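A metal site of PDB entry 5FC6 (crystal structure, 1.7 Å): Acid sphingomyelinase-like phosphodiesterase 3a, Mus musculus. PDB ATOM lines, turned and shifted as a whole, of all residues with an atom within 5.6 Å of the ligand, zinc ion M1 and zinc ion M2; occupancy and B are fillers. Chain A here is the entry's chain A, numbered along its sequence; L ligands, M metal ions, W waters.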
ATOM      1  N   ASP A  30     -15.346 -17.248  26.218  1.00  0.00           N
ATOM      2  CA  ASP A  30     -14.529 -16.036  26.222  1.00  0.00           C
ATOM      3  C   ASP A  30     -14.144 -15.647  27.648  1.00  0.00           C
ATOM      4  O   ASP A  30     -14.433 -14.548  28.123  1.00  0.00           O
ATOM      5  CB  ASP A  30     -15.246 -14.907  25.487  1.00  0.00           C
ATOM      6  CG  ASP A  30     -15.297 -15.158  23.972  1.00  0.00           C
ATOM      7  OD1 ASP A  30     -16.315 -15.729  23.507  1.00  0.00           O
ATOM      8  OD2 ASP A  30     -14.313 -14.811  23.272  1.00  0.00           O
ATOM      9  N   HIS A  32     -11.000 -15.382  28.887  1.00  0.00           N
ATOM     10  CA  HIS A  32      -9.877 -14.432  28.787  1.00  0.00           C
ATOM     11  C   HIS A  32      -9.282 -14.116  30.159  1.00  0.00           C
ATOM     12  O   HIS A  32      -9.325 -12.994  30.643  1.00  0.00           O
ATOM     13  CB  HIS A  32     -10.297 -13.127  28.092  1.00  0.00           C
ATOM     14  CG  HIS A  32     -10.623 -13.292  26.644  1.00  0.00           C
ATOM     15  ND1 HIS A  32      -9.674 -13.555  25.676  1.00  0.00           N
ATOM     16  CD2 HIS A  32     -11.812 -13.195  26.004  1.00  0.00           C
ATOM     17  CE1 HIS A  32     -10.269 -13.606  24.486  1.00  0.00           C
ATOM     18  NE2 HIS A  32     -11.559 -13.392  24.662  1.00  0.00           N
ATOM     19  N   ASP A  95     -11.327 -19.071  23.748  1.00  0.00           N
ATOM     20  CA  ASP A  95     -10.663 -17.785  24.021  1.00  0.00           C
ATOM     21  C   ASP A  95     -10.272 -17.599  25.483  1.00  0.00           C
ATOM     22  O   ASP A  95     -10.881 -16.806  26.218  1.00  0.00           O
ATOM     23  CB  ASP A  95     -11.549 -16.623  23.553  1.00  0.00           C
ATOM     24  CG  ASP A  95     -11.123 -16.055  22.215  1.00  0.00           C
ATOM     25  OD1 ASP A  95     -10.257 -16.655  21.552  1.00  0.00           O
ATOM     26  OD2 ASP A  95     -11.656 -14.956  21.869  1.00  0.00           O
ATOM     27  N   HIS A  99      -5.981 -10.443  26.191  1.00  0.00           N
ATOM     28  CA  HIS A  99      -5.687  -9.556  25.070  1.00  0.00           C
ATOM     29  C   HIS A  99      -4.430  -8.749  25.395  1.00  0.00           C
ATOM     30  O   HIS A  99      -4.500  -7.653  25.977  1.00  0.00           O
ATOM     31  CB  HIS A  99      -6.845  -8.612  24.803  1.00  0.00           C
ATOM     32  CG  HIS A  99      -8.127  -9.308  24.430  1.00  0.00           C
ATOM     33  ND1 HIS A  99      -8.985  -9.822  25.387  1.00  0.00           N
ATOM     34  CD2 HIS A  99      -8.697  -9.555  23.228  1.00  0.00           C
ATOM     35  CE1 HIS A  99     -10.038 -10.364  24.772  1.00  0.00           C
ATOM     36  NE2 HIS A  99      -9.888 -10.221  23.473  1.00  0.00           N
ATOM     37  N   GLY A 135     -10.766 -21.019  20.454  1.00  0.00           N
ATOM     38  CA  GLY A 135     -10.922 -19.636  20.004  1.00  0.00           C
ATOM     39  C   GLY A 135      -9.660 -19.135  19.310  1.00  0.00           C
ATOM     40  O   GLY A 135      -8.607 -19.766  19.304  1.00  0.00           O
ATOM     41  N   ASN A 136      -9.774 -17.935  18.727  1.00  0.00           N
ATOM     42  CA  ASN A 136      -8.654 -17.389  17.969  1.00  0.00           C
ATOM     43  C   ASN A 136      -7.499 -16.965  18.871  1.00  0.00           C
ATOM     44  O   ASN A 136      -6.356 -16.904  18.403  1.00  0.00           O
ATOM     45  CB  ASN A 136      -9.136 -16.215  17.091  1.00  0.00           C
ATOM     46  CG  ASN A 136      -9.873 -15.135  17.894  1.00  0.00           C
ATOM     47  OD1 ASN A 136     -10.932 -15.378  18.471  1.00  0.00           O
ATOM     48  ND2 ASN A 136      -9.264 -13.961  17.997  1.00  0.00           N
ATOM     49  N   HIS A 137      -7.756 -16.680  20.144  1.00  0.00           N
ATOM     50  CA  HIS A 137      -6.680 -16.385  21.067  1.00  0.00           C
ATOM     51  C   HIS A 137      -6.083 -17.651  21.655  1.00  0.00           C
ATOM     52  O   HIS A 137      -5.089 -17.561  22.392  1.00  0.00           O
ATOM     53  CB  HIS A 137      -7.172 -15.465  22.184  1.00  0.00           C
ATOM     54  CG  HIS A 137      -7.448 -14.073  21.721  1.00  0.00           C
ATOM     55  ND1 HIS A 137      -6.477 -13.086  21.725  1.00  0.00           N
ATOM     56  CD2 HIS A 137      -8.563 -13.501  21.194  1.00  0.00           C
ATOM     57  CE1 HIS A 137      -7.004 -11.959  21.242  1.00  0.00           C
ATOM     58  NE2 HIS A 137      -8.265 -12.186  20.931  1.00  0.00           N
ATOM     59  N   GLN A 142      -1.658 -15.205  18.174  1.00  0.00           N
ATOM     60  CA  GLN A 142      -3.105 -15.236  18.083  1.00  0.00           C
ATOM     61  C   GLN A 142      -3.543 -15.225  16.630  1.00  0.00           C
ATOM     62  O   GLN A 142      -2.888 -14.656  15.750  1.00  0.00           O
ATOM     63  CB  GLN A 142      -3.723 -14.044  18.833  1.00  0.00           C
ATOM     64  CG  GLN A 142      -3.509 -12.682  18.215  1.00  0.00           C
ATOM     65  CD  GLN A 142      -4.371 -11.618  18.890  1.00  0.00           C
ATOM     66  OE1 GLN A 142      -4.052 -11.099  19.969  1.00  0.00           O
ATOM     67  NE2 GLN A 142      -5.514 -11.310  18.264  1.00  0.00           N
ATOM     68  N   ASP A 143      -4.670 -15.897  16.396  1.00  0.00           N
ATOM     69  CA  ASP A 143      -5.426 -15.953  15.160  1.00  0.00           C
ATOM     70  C   ASP A 143      -4.762 -16.855  14.114  1.00  0.00           C
ATOM     71  O   ASP A 143      -5.393 -17.132  13.102  1.00  0.00           O
ATOM     72  CB  ASP A 143      -5.648 -14.572  14.526  1.00  0.00           C
ATOM     73  CG  ASP A 143      -6.207 -13.547  15.488  1.00  0.00           C
ATOM     74  OD1 ASP A 143      -6.967 -13.908  16.420  1.00  0.00           O
ATOM     75  OD2 ASP A 143      -5.891 -12.345  15.306  1.00  0.00           O
ATOM     76  N   TYR A 199     -11.288 -17.167   9.905  1.00  0.00           N
ATOM     77  CA  TYR A 199     -11.283 -15.804  10.467  1.00  0.00           C
ATOM     78  C   TYR A 199     -10.251 -14.944   9.737  1.00  0.00           C
ATOM     79  O   TYR A 199      -9.130 -15.366   9.455  1.00  0.00           O
ATOM     80  CB  TYR A 199     -10.996 -15.916  11.968  1.00  0.00           C
ATOM     81  CG  TYR A 199     -10.989 -14.654  12.756  1.00  0.00           C
ATOM     82  CD1 TYR A 199     -12.020 -13.715  12.648  1.00  0.00           C
ATOM     83  CD2 TYR A 199      -9.990 -14.422  13.693  1.00  0.00           C
ATOM     84  CE1 TYR A 199     -12.015 -12.591  13.404  1.00  0.00           C
ATOM     85  CE2 TYR A 199      -9.972 -13.277  14.454  1.00  0.00           C
ATOM     86  CZ  TYR A 199     -10.985 -12.367  14.308  1.00  0.00           C
ATOM     87  OH  TYR A 199     -10.972 -11.234  15.073  1.00  0.00           O
ATOM     88  N   HIS A 237     -16.222 -21.008  17.923  1.00  0.00           N
ATOM     89  CA  HIS A 237     -15.876 -19.703  18.473  1.00  0.00           C
ATOM     90  C   HIS A 237     -16.409 -18.550  17.616  1.00  0.00           C
ATOM     91  O   HIS A 237     -17.312 -17.824  18.040  1.00  0.00           O
ATOM     92  CB  HIS A 237     -14.364 -19.593  18.651  1.00  0.00           C
ATOM     93  CG  HIS A 237     -13.971 -18.313  19.312  1.00  0.00           C
ATOM     94  ND1 HIS A 237     -14.348 -18.014  20.611  1.00  0.00           N
ATOM     95  CD2 HIS A 237     -13.324 -17.232  18.845  1.00  0.00           C
ATOM     96  CE1 HIS A 237     -13.901 -16.805  20.912  1.00  0.00           C
ATOM     97  NE2 HIS A 237     -13.266 -16.317  19.870  1.00  0.00           N
ATOM     98  N   VAL A 238     -15.837 -18.346  16.433  1.00  0.00           N
ATOM     99  CA  VAL A 238     -16.270 -17.239  15.574  1.00  0.00           C
ATOM    100  C   VAL A 238     -17.588 -17.621  14.910  1.00  0.00           C
ATOM    101  O   VAL A 238     -17.694 -18.736  14.380  1.00  0.00           O
ATOM    102  CB  VAL A 238     -15.226 -16.891  14.522  1.00  0.00           C
ATOM    103  CG1 VAL A 238     -15.652 -15.636  13.727  1.00  0.00           C
ATOM    104  CG2 VAL A 238     -13.875 -16.680  15.165  1.00  0.00           C
ATOM    105  N   TYR A 245     -22.739  -4.681  14.538  1.00  0.00           N
ATOM    106  CA  TYR A 245     -22.348  -3.301  14.857  1.00  0.00           C
ATOM    107  C   TYR A 245     -21.606  -2.615  13.726  1.00  0.00           C
ATOM    108  O   TYR A 245     -21.178  -1.474  13.886  1.00  0.00           O
ATOM    109  CB  TYR A 245     -21.467  -3.276  16.113  1.00  0.00           C
ATOM    110  CG  TYR A 245     -20.196  -4.108  15.969  1.00  0.00           C
ATOM    111  CD1 TYR A 245     -20.177  -5.437  16.387  1.00  0.00           C
ATOM    112  CD2 TYR A 245     -19.045  -3.591  15.385  1.00  0.00           C
ATOM    113  CE1 TYR A 245     -19.071  -6.211  16.257  1.00  0.00           C
ATOM    114  CE2 TYR A 245     -17.896  -4.378  15.240  1.00  0.00           C
ATOM    115  CZ  TYR A 245     -17.926  -5.697  15.681  1.00  0.00           C
ATOM    116  OH  TYR A 245     -16.830  -6.513  15.578  1.00  0.00           O
ATOM    117  N   HIS A 278     -17.033 -15.331  20.706  1.00  0.00           N
ATOM    118  CA  HIS A 278     -16.182 -14.344  20.034  1.00  0.00           C
ATOM    119  C   HIS A 278     -16.655 -12.891  20.047  1.00  0.00           C
ATOM    120  O   HIS A 278     -15.821 -11.967  20.086  1.00  0.00           O
ATOM    121  CB  HIS A 278     -15.972 -14.767  18.573  1.00  0.00           C
ATOM    122  CG  HIS A 278     -15.056 -13.861  17.811  1.00  0.00           C
ATOM    123  ND1 HIS A 278     -13.694 -13.774  18.057  1.00  0.00           N
ATOM    124  CD2 HIS A 278     -15.299 -13.036  16.763  1.00  0.00           C
ATOM    125  CE1 HIS A 278     -13.159 -12.907  17.215  1.00  0.00           C
ATOM    126  NE2 HIS A 278     -14.109 -12.434  16.429  1.00  0.00           N
ATOM    127  N   THR A 279     -17.956 -12.631  19.942  1.00  0.00           N
ATOM    128  CA  THR A 279     -18.375 -11.243  19.850  1.00  0.00           C
ATOM    129  C   THR A 279     -18.483 -10.579  21.222  1.00  0.00           C
ATOM    130  O   THR A 279     -18.531  -9.350  21.315  1.00  0.00           O
ATOM    131  CB  THR A 279     -19.743 -11.139  19.157  1.00  0.00           C
ATOM    132  OG1 THR A 279     -20.723 -11.598  20.056  1.00  0.00           O
ATOM    133  CG2 THR A 279     -19.795 -11.941  17.877  1.00  0.00           C
ATOM    134  N   HIS A 280     -18.534 -11.373  22.277  1.00  0.00           N
ATOM    135  CA  HIS A 280     -18.699 -10.882  23.643  1.00  0.00           C
ATOM    136  C   HIS A 280     -20.018 -10.192  23.850  1.00  0.00           C
ATOM    137  O   HIS A 280     -20.185  -9.382  24.772  1.00  0.00           O
ATOM    138  CB  HIS A 280     -17.537  -9.943  24.059  1.00  0.00           C
ATOM    139  CG  HIS A 280     -16.180 -10.583  24.074  1.00  0.00           C
ATOM    140  ND1 HIS A 280     -15.125 -10.058  24.797  1.00  0.00           N
ATOM    141  CD2 HIS A 280     -15.701 -11.683  23.459  1.00  0.00           C
ATOM    142  CE1 HIS A 280     -14.052 -10.799  24.595  1.00  0.00           C
ATOM    143  NE2 HIS A 280     -14.371 -11.803  23.803  1.00  0.00           N
ATOM    144  N   ARG A 281     -21.000 -10.503  23.020  1.00  0.00           N
ATOM    145  CA  ARG A 281     -22.308  -9.872  23.097  1.00  0.00           C
ATOM    146  C   ARG A 281     -23.376 -10.958  23.053  1.00  0.00           C
ATOM    147  O   ARG A 281     -23.123 -12.071  22.612  1.00  0.00           O
ATOM    148  CB  ARG A 281     -22.530  -8.888  21.937  1.00  0.00           C
ATOM    149  CG  ARG A 281     -21.539  -7.752  21.887  1.00  0.00           C
ATOM    150  CD  ARG A 281     -21.788  -6.723  22.982  1.00  0.00           C
ATOM    151  NE  ARG A 281     -20.824  -5.633  22.907  1.00  0.00           N
ATOM    152  CZ  ARG A 281     -19.667  -5.596  23.555  1.00  0.00           C
ATOM    153  NH1 ARG A 281     -19.290  -6.582  24.361  1.00  0.00           N
ATOM    154  NH2 ARG A 281     -18.867  -4.568  23.385  1.00  0.00           N
ATOM    155  N   THR A 305     -15.359 -12.282  30.426  1.00  0.00           N
ATOM    156  CA  THR A 305     -14.569 -11.043  30.499  1.00  0.00           C
ATOM    157  C   THR A 305     -15.443  -9.831  30.161  1.00  0.00           C
ATOM    158  O   THR A 305     -16.306  -9.895  29.255  1.00  0.00           O
ATOM    159  CB  THR A 305     -13.335 -11.082  29.583  1.00  0.00           C
ATOM    160  OG1 THR A 305     -12.553  -9.903  29.791  1.00  0.00           O
ATOM    161  CG2 THR A 305     -13.716 -11.135  28.079  1.00  0.00           C
ATOM    162  N   GLN A 312     -14.019   2.311  22.794  1.00  0.00           N
ATOM    163  CA  GLN A 312     -15.378   1.818  22.793  1.00  0.00           C
ATOM    164  C   GLN A 312     -16.168   2.465  23.906  1.00  0.00           C
ATOM    165  O   GLN A 312     -15.685   2.597  25.028  1.00  0.00           O
ATOM    166  CB  GLN A 312     -15.415   0.291  22.981  1.00  0.00           C
ATOM    167  CG  GLN A 312     -14.796  -0.503  21.860  1.00  0.00           C
ATOM    168  CD  GLN A 312     -14.717  -1.996  22.215  1.00  0.00           C
ATOM    169  OE1 GLN A 312     -13.657  -2.503  22.579  1.00  0.00           O
ATOM    170  NE2 GLN A 312     -15.852  -2.675  22.149  1.00  0.00           N
ATOM    171  N   TYR A 395     -28.133  -6.992  24.686  1.00  0.00           N
ATOM    172  CA  TYR A 395     -26.977  -7.192  23.819  1.00  0.00           C
ATOM    173  C   TYR A 395     -25.671  -6.917  24.572  1.00  0.00           C
ATOM    174  O   TYR A 395     -24.696  -7.671  24.451  1.00  0.00           O
ATOM    175  CB  TYR A 395     -27.157  -6.297  22.588  1.00  0.00           C
ATOM    176  CG  TYR A 395     -25.988  -6.162  21.647  1.00  0.00           C
ATOM    177  CD1 TYR A 395     -25.634  -7.193  20.787  1.00  0.00           C
ATOM    178  CD2 TYR A 395     -25.266  -4.969  21.568  1.00  0.00           C
ATOM    179  CE1 TYR A 395     -24.556  -7.061  19.899  1.00  0.00           C
ATOM    180  CE2 TYR A 395     -24.180  -4.838  20.685  1.00  0.00           C
ATOM    181  CZ  TYR A 395     -23.841  -5.870  19.851  1.00  0.00           C
ATOM    182  OH  TYR A 395     -22.781  -5.728  18.993  1.00  0.00           O
HETATM  183  P1  LIG L   1     -11.968 -11.953  20.697  1.00  0.00           P
HETATM  184  O1  LIG L   1     -11.326 -11.625  22.015  1.00  0.00           O
HETATM  185  O2  LIG L   1     -11.126 -12.684  19.711  1.00  0.00           O
HETATM  186  O3  LIG L   1     -13.213 -12.862  21.048  1.00  0.00           O
HETATM  187  C1  LIG L   1     -12.698 -10.484  19.873  1.00  0.00           C
HETATM  188  P2  LIG L   1     -11.360  -9.211  19.830  1.00  0.00           P
HETATM  189  O4  LIG L   1     -11.448  -8.397  21.111  1.00  0.00           O
HETATM  190  O5  LIG L   1     -10.076 -10.010  19.771  1.00  0.00           O
HETATM  191  O6  LIG L   1     -11.637  -8.167  18.581  1.00  0.00           O
HETATM  192  C2  LIG L   1     -11.567  -8.477  17.224  1.00  0.00           C
HETATM  193  C3  LIG L   1     -11.498  -7.179  16.460  1.00  0.00           C
HETATM  194  O7  LIG L   1     -12.670  -6.672  16.223  1.00  0.00           O
HETATM  195  C4  LIG L   1     -10.677  -6.019  17.357  1.00  0.00           C
HETATM  196  O8  LIG L   1      -9.920  -5.160  16.458  1.00  0.00           O
HETATM  197  C5  LIG L   1     -11.561  -5.336  17.992  1.00  0.00           C
HETATM  198  O9  LIG L   1     -11.101  -3.921  18.167  1.00  0.00           O
HETATM  199  C6  LIG L   1     -12.854  -5.379  17.099  1.00  0.00           C
HETATM  200  N1  LIG L   1     -13.998  -5.457  17.762  1.00  0.00           N
HETATM  201  C7  LIG L   1     -14.438  -6.570  18.328  1.00  0.00           C
HETATM  202  N2  LIG L   1     -15.620  -6.369  18.888  1.00  0.00           N
HETATM  203  C8  LIG L   1     -15.985  -5.101  18.696  1.00  0.00           C
HETATM  204  C9  LIG L   1     -17.124  -4.335  19.053  1.00  0.00           C
HETATM  205  N3  LIG L   1     -18.204  -4.980  19.798  1.00  0.00           N
HETATM  206  N4  LIG L   1     -17.192  -3.050  18.686  1.00  0.00           N
HETATM  207  C10 LIG L   1     -16.183  -2.503  17.994  1.00  0.00           C
HETATM  208  N5  LIG L   1     -15.100  -3.212  17.647  1.00  0.00           N
HETATM  209  C11 LIG L   1     -14.965  -4.512  17.977  1.00  0.00           C
HETATM  210 ZN    ZN M   1     -12.353 -14.489  19.653  1.00  0.00          ZN
HETATM  211 ZN    ZN M   2     -12.980 -13.331  23.093  1.00  0.00          ZN
HETATM  212  O   HOH W   1     -14.767  -5.668  14.214  1.00  0.00           O
HETATM  213  O   HOH W   2     -18.895  -7.739  19.145  1.00  0.00           O
HETATM  214  O   HOH W   3     -15.460  -9.558  18.883  1.00  0.00           O
HETATM  215  O   HOH W   4     -20.795  -4.097  20.362  1.00  0.00           O
HETATM  216  O   HOH W   5      -7.455  -9.272  19.229  1.00  0.00           O
HETATM  217  O   HOH W   6     -19.221  -0.795  17.983  1.00  0.00           O
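The side-chain carboxylate (OD2) of Asp 30 is bound to zinc ion M2, 2.0 Å away.
An oxygen (O3) of the ligand binds zinc ion M2 (2.1 Å).
Zinc ion M2 is bound by a ring nitrogen (NE2) of His 32 (2.1 Å).
NE2 of His 280 is bound to zinc ion M2, 2.2 Å away.
The side-chain carboxylate (OD2) of Asp 95 binds zinc ion M2 (2.4 Å).
Slightly farther from zinc ion M2 lies O1 of the ligand (2.6 Å).
An oxygen (O1) of the ligand is in hydrogen-bond range of a ring nitrogen (NE2) of His 99 (2.5 Å).
O5 of the ligand sits at hydrogen-bond distance from NE2 of His 137 (3.1 Å).
Of the 20 residues printed, 4 come within 4 Å of zinc ion M1.
The nearest printed residue that does not touch zinc ion M1 is Asp 30 (4.1 Å).
Water W5 lies within hydrogen-bond range of O5 of the ligand (2.8 Å), NE2 of Gln 142 (3.0 Å) and NE2 of His 137 (3.5 Å).
Water W4 lies within hydrogen-bond range of a nitrogen (N3) of the ligand (2.8 Å), the side-chain hydroxyl of Tyr 395 (2.9 Å) and the guanidinium group of Arg 281 (3.0 Å).
Water W2 lies within hydrogen-bond range of O of Thr 279 and N3 of the ligand.
Water W1 lies within hydrogen-bond range of the side-chain hydroxyl of Tyr 245 (2.6 Å) and an oxygen (O7) of the ligand (3.1 Å).
Water W3 bridges the backbone carbonyl oxygen of His 278 and a nitrogen (N2) of the ligand.
Zinc ion M1 is bound by OD1 of Asn 136, 2.1 Å away.
NE2 of His 237 binds zinc ion M1 (2.1 Å).
O2 of the ligand binds zinc ion M1 (2.2 Å).
Zinc ion M1 is bound by ND1 of His 278.
Zinc ion M1 is bound by O3 of the ligand (2.3 Å).
OD2 of Asp 95 binds zinc ion M1, at 2.4 Å.
The side-chain carboxylate (OD1) of Asp 30 is in hydrogen-bond range of the backbone NH (N) of His 278, at 2.9 Å.
The backbone NH of Thr 305 sits at hydrogen-bond distance from the backbone carbonyl oxygen of Asp 30, at 3.4 Å.
ND2 of Asn 136 is in hydrogen-bond range of OD1 of Asp 143 (2.8 Å).
OD1 of Asp 95 lies within hydrogen-bond range of N of His 137, 2.9 Å away.
The backbone NH of Arg 281 lies close to the side-chain hydroxyl of Thr 279, at 3.2 Å.
Four residues have an atom within 4 Å of zinc ion M2: Asp 30, His 32, Asp 95 and His 280.
Along chain A the residues within 4 Å of zinc ion M2 span positions 30 to 280.
OH of Tyr 199 touches C2 of the ligand, at 3.5 Å.
OH of Tyr 245 touches C8 of the ligand (3.5 Å).
Arg 281 touches the ligand (NH2 to N3, 3.7 Å).
Gln 312 touches the ligand (NE2 to N4, 3.7 Å).
Hydrophobic or aromatic side chains within 4 Å of the ligand: His 32, His 99, His 137, Tyr 245, His 278 and His 280.
13 residues have an atom within 4 Å of the ligand: Asp 30, His 32, Asp 95, His 99, Asn 136, His 137, Tyr 199, His 237, Tyr 245, His 278, His 280, Arg 281 and Gln 312.
The nearest printed residue that does not touch the ligand is Thr 279 (4.6 Å).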
